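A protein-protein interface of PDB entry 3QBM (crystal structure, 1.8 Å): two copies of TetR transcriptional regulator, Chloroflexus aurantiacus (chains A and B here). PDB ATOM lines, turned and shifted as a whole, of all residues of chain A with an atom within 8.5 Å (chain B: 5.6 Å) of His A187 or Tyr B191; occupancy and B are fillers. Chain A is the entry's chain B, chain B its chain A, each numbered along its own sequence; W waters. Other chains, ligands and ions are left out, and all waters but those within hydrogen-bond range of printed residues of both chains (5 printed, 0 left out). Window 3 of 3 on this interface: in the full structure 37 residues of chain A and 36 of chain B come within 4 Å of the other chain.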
ATOM      1  N   LEU A  88      -0.119   4.059   8.544  1.00  0.00           N
ATOM      2  CA  LEU A  88      -1.158   3.036   8.744  1.00  0.00           C
ATOM      3  C   LEU A  88      -0.607   1.871   9.550  1.00  0.00           C
ATOM      4  O   LEU A  88      -1.285   1.325  10.434  1.00  0.00           O
ATOM      5  CB  LEU A  88      -1.699   2.459   7.451  1.00  0.00           C
ATOM      6  CG  LEU A  88      -2.152   3.401   6.348  1.00  0.00           C
ATOM      7  CD1 LEU A  88      -2.527   2.570   5.127  1.00  0.00           C
ATOM      8  CD2 LEU A  88      -3.296   4.346   6.845  1.00  0.00           C
ATOM      9  N   ARG A  92      -1.835  -0.365  12.776  1.00  0.00           N
ATOM     10  CA  ARG A  92      -1.997  -1.801  12.588  1.00  0.00           C
ATOM     11  C   ARG A  92      -1.321  -2.542  13.754  1.00  0.00           C
ATOM     12  O   ARG A  92      -1.867  -3.491  14.327  1.00  0.00           O
ATOM     13  CB  ARG A  92      -1.361  -2.210  11.245  1.00  0.00           C
ATOM     14  CG  ARG A  92      -1.579  -3.631  10.790  1.00  0.00           C
ATOM     15  CD  ARG A  92      -0.505  -3.992   9.780  1.00  0.00           C
ATOM     16  NE  ARG A  92      -0.967  -4.965   8.797  1.00  0.00           N
ATOM     17  CZ  ARG A  92      -0.242  -5.384   7.766  1.00  0.00           C
ATOM     18  NH1 ARG A  92       0.983  -4.903   7.570  1.00  0.00           N
ATOM     19  NH2 ARG A  92      -0.748  -6.272   6.920  1.00  0.00           N
ATOM     20  N   LEU A 160      -9.850  10.515   6.815  1.00  0.00           N
ATOM     21  CA  LEU A 160     -10.220   9.109   6.485  1.00  0.00           C
ATOM     22  C   LEU A 160      -9.277   8.082   7.156  1.00  0.00           C
ATOM     23  O   LEU A 160      -9.739   7.144   7.784  1.00  0.00           O
ATOM     24  CB  LEU A 160     -10.275   8.872   4.985  1.00  0.00           C
ATOM     25  CG  LEU A 160     -10.610   7.456   4.501  1.00  0.00           C
ATOM     26  CD1 LEU A 160     -12.007   7.077   4.939  1.00  0.00           C
ATOM     27  CD2 LEU A 160     -10.430   7.336   2.957  1.00  0.00           C
ATOM     28  N   THR A 164     -10.655   5.528  10.099  1.00  0.00           N
ATOM     29  CA  THR A 164     -10.590   4.102   9.801  1.00  0.00           C
ATOM     30  C   THR A 164      -9.689   3.345  10.750  1.00  0.00           C
ATOM     31  O   THR A 164     -10.081   2.331  11.276  1.00  0.00           O
ATOM     32  CB  THR A 164     -10.162   3.847   8.323  1.00  0.00           C
ATOM     33  OG1 THR A 164     -10.999   4.610   7.413  1.00  0.00           O
ATOM     34  CG2 THR A 164     -10.240   2.369   7.988  1.00  0.00           C
ATOM     35  N   MET A 165      -8.475   3.836  10.979  1.00  0.00           N
ATOM     36  CA  MET A 165      -7.549   3.090  11.789  1.00  0.00           C
ATOM     37  C   MET A 165      -7.990   3.102  13.239  1.00  0.00           C
ATOM     38  O   MET A 165      -7.908   2.039  13.884  1.00  0.00           O
ATOM     39  CB  MET A 165      -6.114   3.607  11.609  1.00  0.00           C
ATOM     40  CG  MET A 165      -5.583   3.443  10.145  1.00  0.00           C
ATOM     41  SD  MET A 165      -5.779   1.674   9.345  1.00  0.00           S
ATOM     42  CE  MET A 165      -4.783   0.550  10.530  1.00  0.00           C
ATOM     43  N   PRO A 180      -9.678  -6.803  12.417  1.00  0.00           N
ATOM     44  CA  PRO A 180     -10.175  -5.496  11.931  1.00  0.00           C
ATOM     45  C   PRO A 180      -9.067  -4.538  11.522  1.00  0.00           C
ATOM     46  O   PRO A 180      -9.202  -3.803  10.533  1.00  0.00           O
ATOM     47  CB  PRO A 180     -10.910  -4.942  13.148  1.00  0.00           C
ATOM     48  CG  PRO A 180     -11.200  -6.090  13.981  1.00  0.00           C
ATOM     49  CD  PRO A 180     -10.095  -7.038  13.797  1.00  0.00           C
ATOM     50  N   LEU A 181      -7.959  -4.579  12.251  1.00  0.00           N
ATOM     51  CA  LEU A 181      -6.803  -3.705  11.953  1.00  0.00           C
ATOM     52  C   LEU A 181      -6.102  -4.138  10.664  1.00  0.00           C
ATOM     53  O   LEU A 181      -5.739  -3.307   9.824  1.00  0.00           O
ATOM     54  CB  LEU A 181      -5.862  -3.651  13.169  1.00  0.00           C
ATOM     55  CG  LEU A 181      -6.229  -2.580  14.193  1.00  0.00           C
ATOM     56  CD1 LEU A 181      -5.470  -2.795  15.514  1.00  0.00           C
ATOM     57  CD2 LEU A 181      -5.965  -1.174  13.664  1.00  0.00           C
ATOM     58  N   GLU A 182      -5.990  -5.451  10.474  1.00  0.00           N
ATOM     59  CA  GLU A 182      -5.441  -5.998   9.233  1.00  0.00           C
ATOM     60  C   GLU A 182      -6.273  -5.587   8.038  1.00  0.00           C
ATOM     61  O   GLU A 182      -5.736  -5.197   7.024  1.00  0.00           O
ATOM     62  CB  GLU A 182      -5.338  -7.524   9.265  1.00  0.00           C
ATOM     63  CG  GLU A 182      -4.240  -8.078  10.162  1.00  0.00           C
ATOM     64  CD  GLU A 182      -2.847  -7.574   9.794  1.00  0.00           C
ATOM     65  OE1 GLU A 182      -2.542  -7.422   8.585  1.00  0.00           O
ATOM     66  OE2 GLU A 182      -2.070  -7.318  10.727  1.00  0.00           O
ATOM     67  N   HIS A 183      -7.592  -5.680   8.161  1.00  0.00           N
ATOM     68  CA  HIS A 183      -8.463  -5.307   7.053  1.00  0.00           C
ATOM     69  C   HIS A 183      -8.448  -3.829   6.752  1.00  0.00           C
ATOM     70  O   HIS A 183      -8.470  -3.449   5.579  1.00  0.00           O
ATOM     71  CB  HIS A 183      -9.901  -5.714   7.309  1.00  0.00           C
ATOM     72  CG  HIS A 183     -10.071  -7.187   7.486  1.00  0.00           C
ATOM     73  ND1 HIS A 183      -9.270  -8.101   6.834  1.00  0.00           N
ATOM     74  CD2 HIS A 183     -10.952  -7.904   8.218  1.00  0.00           C
ATOM     75  CE1 HIS A 183      -9.636  -9.327   7.183  1.00  0.00           C
ATOM     76  NE2 HIS A 183     -10.664  -9.237   8.009  1.00  0.00           N
ATOM     77  N   ALA A 184      -8.461  -3.010   7.797  1.00  0.00           N
ATOM     78  CA  ALA A 184      -8.467  -1.559   7.645  1.00  0.00           C
ATOM     79  C   ALA A 184      -7.151  -1.115   6.983  1.00  0.00           C
ATOM     80  O   ALA A 184      -7.155  -0.311   6.053  1.00  0.00           O
ATOM     81  CB  ALA A 184      -8.689  -0.838   9.034  1.00  0.00           C
ATOM     82  N   TYR A 185      -6.043  -1.675   7.446  1.00  0.00           N
ATOM     83  CA  TYR A 185      -4.735  -1.454   6.837  1.00  0.00           C
ATOM     84  C   TYR A 185      -4.718  -1.818   5.357  1.00  0.00           C
ATOM     85  O   TYR A 185      -4.313  -1.008   4.524  1.00  0.00           O
ATOM     86  CB  TYR A 185      -3.645  -2.208   7.592  1.00  0.00           C
ATOM     87  CG  TYR A 185      -2.312  -2.139   6.939  1.00  0.00           C
ATOM     88  CD1 TYR A 185      -1.431  -1.077   7.221  1.00  0.00           C
ATOM     89  CD2 TYR A 185      -1.916  -3.099   6.006  1.00  0.00           C
ATOM     90  CE1 TYR A 185      -0.178  -0.997   6.582  1.00  0.00           C
ATOM     91  CE2 TYR A 185      -0.678  -3.019   5.374  1.00  0.00           C
ATOM     92  CZ  TYR A 185       0.183  -1.970   5.679  1.00  0.00           C
ATOM     93  OH  TYR A 185       1.387  -1.880   5.050  1.00  0.00           O
ATOM     94  N   THR A 186      -5.172  -3.018   5.013  1.00  0.00           N
ATOM     95  CA  THR A 186      -5.124  -3.483   3.634  1.00  0.00           C
ATOM     96  C   THR A 186      -5.995  -2.623   2.745  1.00  0.00           C
ATOM     97  O   THR A 186      -5.604  -2.268   1.650  1.00  0.00           O
ATOM     98  CB  THR A 186      -5.511  -4.970   3.542  1.00  0.00           C
ATOM     99  OG1 THR A 186      -4.437  -5.710   4.136  1.00  0.00           O
ATOM    100  CG2 THR A 186      -5.689  -5.428   2.113  1.00  0.00           C
ATOM    101  N   HIS A 187      -7.177  -2.296   3.241  1.00  0.00           N
ATOM    102  CA  HIS A 187      -8.072  -1.430   2.484  1.00  0.00           C
ATOM    103  C   HIS A 187      -7.431  -0.087   2.125  1.00  0.00           C
ATOM    104  O   HIS A 187      -7.439   0.334   0.967  1.00  0.00           O
ATOM    105  CB  HIS A 187      -9.353  -1.159   3.266  1.00  0.00           C
ATOM    106  CG  HIS A 187     -10.248  -0.196   2.560  1.00  0.00           C
ATOM    107  ND1 HIS A 187     -10.914  -0.539   1.401  1.00  0.00           N
ATOM    108  CD2 HIS A 187     -10.447   1.129   2.734  1.00  0.00           C
ATOM    109  CE1 HIS A 187     -11.573   0.518   0.948  1.00  0.00           C
ATOM    110  NE2 HIS A 187     -11.306   1.544   1.741  1.00  0.00           N
ATOM    111  N   LEU A 188      -6.925   0.604   3.138  1.00  0.00           N
ATOM    112  CA  LEU A 188      -6.345   1.942   2.947  1.00  0.00           C
ATOM    113  C   LEU A 188      -5.030   1.907   2.168  1.00  0.00           C
ATOM    114  O   LEU A 188      -4.761   2.811   1.350  1.00  0.00           O
ATOM    115  CB  LEU A 188      -6.182   2.672   4.284  1.00  0.00           C
ATOM    116  CG  LEU A 188      -7.437   3.177   4.938  1.00  0.00           C
ATOM    117  CD1 LEU A 188      -7.129   3.746   6.323  1.00  0.00           C
ATOM    118  CD2 LEU A 188      -8.172   4.234   4.016  1.00  0.00           C
ATOM    119  N   ALA A 189      -4.197   0.897   2.406  1.00  0.00           N
ATOM    120  CA  ALA A 189      -2.966   0.765   1.630  1.00  0.00           C
ATOM    121  C   ALA A 189      -3.287   0.571   0.142  1.00  0.00           C
ATOM    122  O   ALA A 189      -2.638   1.134  -0.719  1.00  0.00           O
ATOM    123  CB  ALA A 189      -2.073  -0.395   2.174  1.00  0.00           C
ATOM    124  N   THR A 190      -4.286  -0.257  -0.147  1.00  0.00           N
ATOM    125  CA  THR A 190      -4.702  -0.526  -1.511  1.00  0.00           C
ATOM    126  C   THR A 190      -5.306   0.710  -2.116  1.00  0.00           C
ATOM    127  O   THR A 190      -4.939   1.091  -3.221  1.00  0.00           O
ATOM    128  CB  THR A 190      -5.694  -1.691  -1.585  1.00  0.00           C
ATOM    129  OG1 THR A 190      -5.074  -2.846  -0.998  1.00  0.00           O
ATOM    130  CG2 THR A 190      -6.142  -1.962  -3.035  1.00  0.00           C
ATOM    131  N   TYR A 191      -6.183   1.368  -1.357  1.00  0.00           N
ATOM    132  CA  TYR A 191      -6.823   2.604  -1.821  1.00  0.00           C
ATOM    133  C   TYR A 191      -5.782   3.671  -2.193  1.00  0.00           C
ATOM    134  O   TYR A 191      -5.833   4.273  -3.267  1.00  0.00           O
ATOM    135  CB  TYR A 191      -7.728   3.159  -0.746  1.00  0.00           C
ATOM    136  CG  TYR A 191      -8.228   4.567  -1.046  1.00  0.00           C
ATOM    137  CD1 TYR A 191      -9.125   4.811  -2.078  1.00  0.00           C
ATOM    138  CD2 TYR A 191      -7.852   5.631  -0.247  1.00  0.00           C
ATOM    139  CE1 TYR A 191      -9.599   6.112  -2.324  1.00  0.00           C
ATOM    140  CE2 TYR A 191      -8.350   6.918  -0.480  1.00  0.00           C
ATOM    141  CZ  TYR A 191      -9.191   7.145  -1.519  1.00  0.00           C
ATOM    142  OH  TYR A 191      -9.638   8.450  -1.718  1.00  0.00           O
ATOM    143  N   ILE A 192      -4.843   3.882  -1.287  1.00  0.00           N
ATOM    144  CA  ILE A 192      -3.770   4.853  -1.493  1.00  0.00           C
ATOM    145  C   ILE A 192      -2.916   4.530  -2.703  1.00  0.00           C
ATOM    146  O   ILE A 192      -2.612   5.408  -3.520  1.00  0.00           O
ATOM    147  CB  ILE A 192      -2.914   4.997  -0.230  1.00  0.00           C
ATOM    148  CG1 ILE A 192      -3.706   5.780   0.837  1.00  0.00           C
ATOM    149  CG2 ILE A 192      -1.579   5.733  -0.535  1.00  0.00           C
ATOM    150  CD1 ILE A 192      -3.198   5.605   2.263  1.00  0.00           C
ATOM    151  N   THR A 193      -2.527   3.272  -2.830  1.00  0.00           N
ATOM    152  CA  THR A 193      -1.696   2.847  -3.948  1.00  0.00           C
ATOM    153  C   THR A 193      -2.469   3.020  -5.252  1.00  0.00           C
ATOM    154  O   THR A 193      -1.944   3.497  -6.243  1.00  0.00           O
ATOM    155  CB  THR A 193      -1.280   1.363  -3.767  1.00  0.00           C
ATOM    156  OG1 THR A 193      -0.492   1.221  -2.574  1.00  0.00           O
ATOM    157  CG2 THR A 193      -0.445   0.890  -4.956  1.00  0.00           C
ATOM    158  N   GLN A 194      -3.757   2.701  -5.222  1.00  0.00           N
ATOM    159  CA  GLN A 194      -4.536   2.756  -6.430  1.00  0.00           C
ATOM    160  C   GLN A 194      -5.077   4.111  -6.805  1.00  0.00           C
ATOM    161  O   GLN A 194      -5.208   4.368  -7.980  1.00  0.00           O
ATOM    162  CB  GLN A 194      -5.681   1.757  -6.398  1.00  0.00           C
ATOM    163  CG  GLN A 194      -5.206   0.316  -6.365  1.00  0.00           C
ATOM    164  CD  GLN A 194      -6.331  -0.699  -6.395  1.00  0.00           C
ATOM    165  OE1 GLN A 194      -7.455  -0.401  -6.038  1.00  0.00           O
ATOM    166  NE2 GLN A 194      -6.019  -1.904  -6.837  1.00  0.00           N
ATOM    167  N   GLN A 195      -5.370   4.973  -5.830  1.00  0.00           N
ATOM    168  CA  GLN A 195      -6.056   6.237  -6.112  1.00  0.00           C
ATOM    169  C   GLN A 195      -5.270   7.483  -5.711  1.00  0.00           C
ATOM    170  O   GLN A 195      -5.604   8.567  -6.144  1.00  0.00           O
ATOM    171  CB  GLN A 195      -7.459   6.214  -5.464  1.00  0.00           C
ATOM    172  CG  GLN A 195      -8.307   5.048  -5.959  1.00  0.00           C
ATOM    173  CD  GLN A 195      -9.796   5.167  -5.634  1.00  0.00           C
ATOM    174  OE1 GLN A 195     -10.401   6.217  -5.854  1.00  0.00           O
ATOM    175  NE2 GLN A 195     -10.403   4.070  -5.099  1.00  0.00           N
ATOM    176  N   LEU B 157     -15.847  -6.621   4.450  1.00  0.00           N
ATOM    177  CA  LEU B 157     -16.565  -5.363   4.170  1.00  0.00           C
ATOM    178  C   LEU B 157     -17.229  -4.835   5.446  1.00  0.00           C
ATOM    179  O   LEU B 157     -17.158  -3.628   5.770  1.00  0.00           O
ATOM    180  CB  LEU B 157     -17.578  -5.575   3.048  1.00  0.00           C
ATOM    181  CG  LEU B 157     -18.448  -4.370   2.660  1.00  0.00           C
ATOM    182  CD1 LEU B 157     -17.511  -3.222   2.204  1.00  0.00           C
ATOM    183  CD2 LEU B 157     -19.535  -4.712   1.594  1.00  0.00           C
ATOM    184  N   LEU B 160     -14.722  -3.393   7.820  1.00  0.00           N
ATOM    185  CA  LEU B 160     -14.211  -2.104   7.305  1.00  0.00           C
ATOM    186  C   LEU B 160     -15.225  -0.972   7.539  1.00  0.00           C
ATOM    187  O   LEU B 160     -14.861   0.120   8.039  1.00  0.00           O
ATOM    188  CB  LEU B 160     -13.909  -2.215   5.821  1.00  0.00           C
ATOM    189  CG  LEU B 160     -13.521  -0.913   5.118  1.00  0.00           C
ATOM    190  CD1 LEU B 160     -12.159  -0.416   5.646  1.00  0.00           C
ATOM    191  CD2 LEU B 160     -13.474  -1.188   3.593  1.00  0.00           C
ATOM    192  N   THR B 186     -18.836   9.265   2.199  1.00  0.00           N
ATOM    193  CA  THR B 186     -18.572   9.425   0.758  1.00  0.00           C
ATOM    194  C   THR B 186     -17.530   8.414   0.281  1.00  0.00           C
ATOM    195  O   THR B 186     -17.686   7.772  -0.738  1.00  0.00           O
ATOM    196  CB  THR B 186     -18.162  10.886   0.461  1.00  0.00           C
ATOM    197  OG1 THR B 186     -19.288  11.719   0.737  1.00  0.00           O
ATOM    198  CG2 THR B 186     -17.641  11.111  -0.983  1.00  0.00           C
ATOM    199  N   HIS B 187     -16.467   8.270   1.053  1.00  0.00           N
ATOM    200  CA  HIS B 187     -15.445   7.307   0.685  1.00  0.00           C
ATOM    201  C   HIS B 187     -16.013   5.899   0.537  1.00  0.00           C
ATOM    202  O   HIS B 187     -15.809   5.254  -0.480  1.00  0.00           O
ATOM    203  CB  HIS B 187     -14.371   7.235   1.748  1.00  0.00           C
ATOM    204  CG  HIS B 187     -13.377   6.171   1.471  1.00  0.00           C
ATOM    205  ND1 HIS B 187     -12.481   6.267   0.429  1.00  0.00           N
ATOM    206  CD2 HIS B 187     -13.117   4.997   2.097  1.00  0.00           C
ATOM    207  CE1 HIS B 187     -11.736   5.170   0.410  1.00  0.00           C
ATOM    208  NE2 HIS B 187     -12.079   4.405   1.431  1.00  0.00           N
ATOM    209  N   LEU B 188     -16.730   5.429   1.542  1.00  0.00           N
ATOM    210  CA  LEU B 188     -17.286   4.078   1.496  1.00  0.00           C
ATOM    211  C   LEU B 188     -18.413   3.905   0.475  1.00  0.00           C
ATOM    212  O   LEU B 188     -18.493   2.879  -0.184  1.00  0.00           O
ATOM    213  CB  LEU B 188     -17.706   3.593   2.887  1.00  0.00           C
ATOM    214  CG  LEU B 188     -16.523   3.276   3.835  1.00  0.00           C
ATOM    215  CD1 LEU B 188     -17.105   2.945   5.210  1.00  0.00           C
ATOM    216  CD2 LEU B 188     -15.559   2.181   3.310  1.00  0.00           C
ATOM    217  N   ALA B 189     -19.293   4.878   0.348  1.00  0.00           N
ATOM    218  CA  ALA B 189     -20.349   4.792  -0.639  1.00  0.00           C
ATOM    219  C   ALA B 189     -19.755   4.686  -2.033  1.00  0.00           C
ATOM    220  O   ALA B 189     -20.234   3.907  -2.869  1.00  0.00           O
ATOM    221  CB  ALA B 189     -21.290   6.001  -0.534  1.00  0.00           C
ATOM    222  N   THR B 190     -18.697   5.461  -2.275  1.00  0.00           N
ATOM    223  CA  THR B 190     -18.046   5.504  -3.571  1.00  0.00           C
ATOM    224  C   THR B 190     -17.320   4.174  -3.796  1.00  0.00           C
ATOM    225  O   THR B 190     -17.461   3.546  -4.859  1.00  0.00           O
ATOM    226  CB  THR B 190     -17.102   6.715  -3.679  1.00  0.00           C
ATOM    227  OG1 THR B 190     -17.862   7.917  -3.519  1.00  0.00           O
ATOM    228  CG2 THR B 190     -16.428   6.731  -5.035  1.00  0.00           C
ATOM    229  N   TYR B 191     -16.599   3.704  -2.780  1.00  0.00           N
ATOM    230  CA  TYR B 191     -15.884   2.424  -2.874  1.00  0.00           C
ATOM    231  C   TYR B 191     -16.854   1.267  -3.157  1.00  0.00           C
ATOM    232  O   TYR B 191     -16.632   0.459  -4.062  1.00  0.00           O
ATOM    233  CB  TYR B 191     -15.100   2.166  -1.590  1.00  0.00           C
ATOM    234  CG  TYR B 191     -14.680   0.739  -1.405  1.00  0.00           C
ATOM    235  CD1 TYR B 191     -13.684   0.169  -2.226  1.00  0.00           C
ATOM    236  CD2 TYR B 191     -15.222  -0.062  -0.376  1.00  0.00           C
ATOM    237  CE1 TYR B 191     -13.281  -1.164  -2.035  1.00  0.00           C
ATOM    238  CE2 TYR B 191     -14.818  -1.374  -0.193  1.00  0.00           C
ATOM    239  CZ  TYR B 191     -13.850  -1.919  -1.032  1.00  0.00           C
ATOM    240  OH  TYR B 191     -13.433  -3.228  -0.850  1.00  0.00           O
ATOM    241  N   ILE B 192     -17.944   1.222  -2.405  1.00  0.00           N
ATOM    242  CA  ILE B 192     -18.968   0.170  -2.573  1.00  0.00           C
ATOM    243  C   ILE B 192     -19.632   0.266  -3.953  1.00  0.00           C
ATOM    244  O   ILE B 192     -19.779  -0.729  -4.677  1.00  0.00           O
ATOM    245  CB  ILE B 192     -19.974   0.212  -1.407  1.00  0.00           C
ATOM    246  CG1 ILE B 192     -19.312  -0.231  -0.114  1.00  0.00           C
ATOM    247  CG2 ILE B 192     -21.182  -0.682  -1.697  1.00  0.00           C
ATOM    248  CD1 ILE B 192     -20.136   0.160   1.106  1.00  0.00           C
ATOM    249  N   THR B 193     -19.991   1.463  -4.375  1.00  0.00           N
ATOM    250  CA  THR B 193     -20.624   1.614  -5.685  1.00  0.00           C
ATOM    251  C   THR B 193     -19.684   1.242  -6.849  1.00  0.00           C
ATOM    252  O   THR B 193     -20.108   0.624  -7.852  1.00  0.00           O
ATOM    253  CB  THR B 193     -21.078   3.064  -5.863  1.00  0.00           C
ATOM    254  OG1 THR B 193     -22.031   3.363  -4.845  1.00  0.00           O
ATOM    255  CG2 THR B 193     -21.697   3.290  -7.245  1.00  0.00           C
ATOM    256  N   GLN B 194     -18.398   1.557  -6.694  1.00  0.00           N
ATOM    257  CA  GLN B 194     -17.423   1.340  -7.755  1.00  0.00           C
ATOM    258  C   GLN B 194     -16.855  -0.073  -7.799  1.00  0.00           C
ATOM    259  O   GLN B 194     -16.618  -0.608  -8.877  1.00  0.00           O
ATOM    260  CB  GLN B 194     -16.259   2.350  -7.652  1.00  0.00           C
ATOM    261  CG  GLN B 194     -16.672   3.779  -7.952  1.00  0.00           C
ATOM    262  CD  GLN B 194     -15.518   4.762  -7.903  1.00  0.00           C
ATOM    263  OE1 GLN B 194     -14.429   4.450  -7.411  1.00  0.00           O
ATOM    264  NE2 GLN B 194     -15.761   5.976  -8.397  1.00  0.00           N
ATOM    265  N   GLN B 195     -16.636  -0.676  -6.628  1.00  0.00           N
ATOM    266  CA  GLN B 195     -15.949  -1.960  -6.536  1.00  0.00           C
ATOM    267  C   GLN B 195     -16.716  -3.160  -5.994  1.00  0.00           C
ATOM    268  O   GLN B 195     -16.277  -4.267  -6.180  1.00  0.00           O
ATOM    269  CB  GLN B 195     -14.665  -1.798  -5.697  1.00  0.00           C
ATOM    270  CG  GLN B 195     -13.738  -0.688  -6.209  1.00  0.00           C
ATOM    271  CD  GLN B 195     -12.344  -0.724  -5.597  1.00  0.00           C
ATOM    272  OE1 GLN B 195     -11.751  -1.796  -5.444  1.00  0.00           O
ATOM    273  NE2 GLN B 195     -11.790   0.444  -5.300  1.00  0.00           N
ATOM    274  N   VAL B 196     -17.826  -2.941  -5.298  1.00  0.00           N
ATOM    275  CA  VAL B 196     -18.626  -4.019  -4.734  1.00  0.00           C
ATOM    276  C   VAL B 196     -19.869  -4.279  -5.588  1.00  0.00           C
ATOM    277  O   VAL B 196     -20.212  -5.458  -5.858  1.00  0.00           O
ATOM    278  CB  VAL B 196     -18.970  -3.708  -3.289  1.00  0.00           C
ATOM    279  CG1 VAL B 196     -20.050  -4.663  -2.711  1.00  0.00           C
ATOM    280  CG2 VAL B 196     -17.693  -3.766  -2.418  1.00  0.00           C
HETATM  281  O   HOH W   1      -9.329  -2.183  -4.777  1.00  0.00           O
HETATM  282  O   HOH W   2     -10.612  -2.853   0.136  1.00  0.00           O
HETATM  283  O   HOH W   3     -13.374   3.352  -5.244  1.00  0.00           O
HETATM  284  O   HOH W   4      -8.948   1.280  -4.797  1.00  0.00           O
HETATM  285  O   HOH W   5     -12.228   8.481  -1.157  1.00  0.00           O
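The backbone carbonyl oxygen (O) of Leu A160 lies within hydrogen-bond range of the side-chain hydroxyl (OG1) of Thr A164 (2.9 Å).
NE2 of His A187 lies within hydrogen-bond range of NE2 of His B187.
Hydrophobic or aromatic side chains of chain B within 4 Å of the printed part of chain A: Leu B160, His B187 and Tyr B191.
Of the 21 printed residues of chain A, 4 touch a printed residue of chain B.
Printed residues of chain A that touch a printed residue of chain B: Leu A160, His A187, Tyr A191 and Gln A195.
Hydrophobic or aromatic side chains of chain A that line the printed part of chain B: Leu A160, His A187 and Tyr A191.
Among the printed residues, no Asp or Glu carboxylate lies within 4 Å of a Lys or Arg side-chain nitrogen of the other chain.
Leu A160 touches His B187, and with the chains exchanged His A187 touches Leu B160.
His A187 touches its own counterpart, His B187.
His A187 touches Tyr B191, and with the chains exchanged Tyr A191 touches His B187.
Gln B195 touches its own counterpart, Gln A195.
Positions printed for both chains: 160, 186, 187, 188, 189, 190, 191, 192, 193, 194 and 195.
Of the 6 pairs that touch across the chains among the printed residues, 6 have their exchanged pair printed and touching as well.
Leu A160 touches His B187.
Leu B160 touches His A187.
Tyr B191 touches His A187.
His B187 touches Tyr A191 (CE1 to CE1, 3.6 Å).
Gln A195 touches Gln B195 (NE2 to NE2, 3.9 Å).
Printed residues of chain B within 4 Å of Leu A160: His B187.
Tyr A185 touches none of the printed residues of chain B.
His A187 touches just these residues of chain B: Leu B160, His B187 and Tyr B191.
Printed residues of chain B within 4 Å of Gln A195: Gln B195 (3.9 Å).
Tyr B191 touches just one residue of chain A: His A187 (3.8 Å).
Printed residues of chain A within 4 Å of Gln B195: Gln A195 (3.9 Å).
Water W1 lies within hydrogen-bond range of OE1 of Gln B195 (2.5 Å) and OE1 of Gln A194 (2.9 Å).
Water W4 lies within hydrogen-bond range of the side-chain amide oxygen of Gln A194 (2.6 Å), the side-chain amide nitrogen of Gln B195 (3.0 Å) and the side-chain amide nitrogen of Gln A195 (3.2 Å).
Water W3 lies within hydrogen-bond range of OE1 of Gln B194, NE2 of Gln A195 and NE2 of Gln B195.
Water W5 lies within hydrogen-bond range of OH of Tyr A191 and ND1 of His B187.
Water W2 bridges a ring nitrogen (ND1) of His A187 and the side-chain hydroxyl of Tyr B191.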
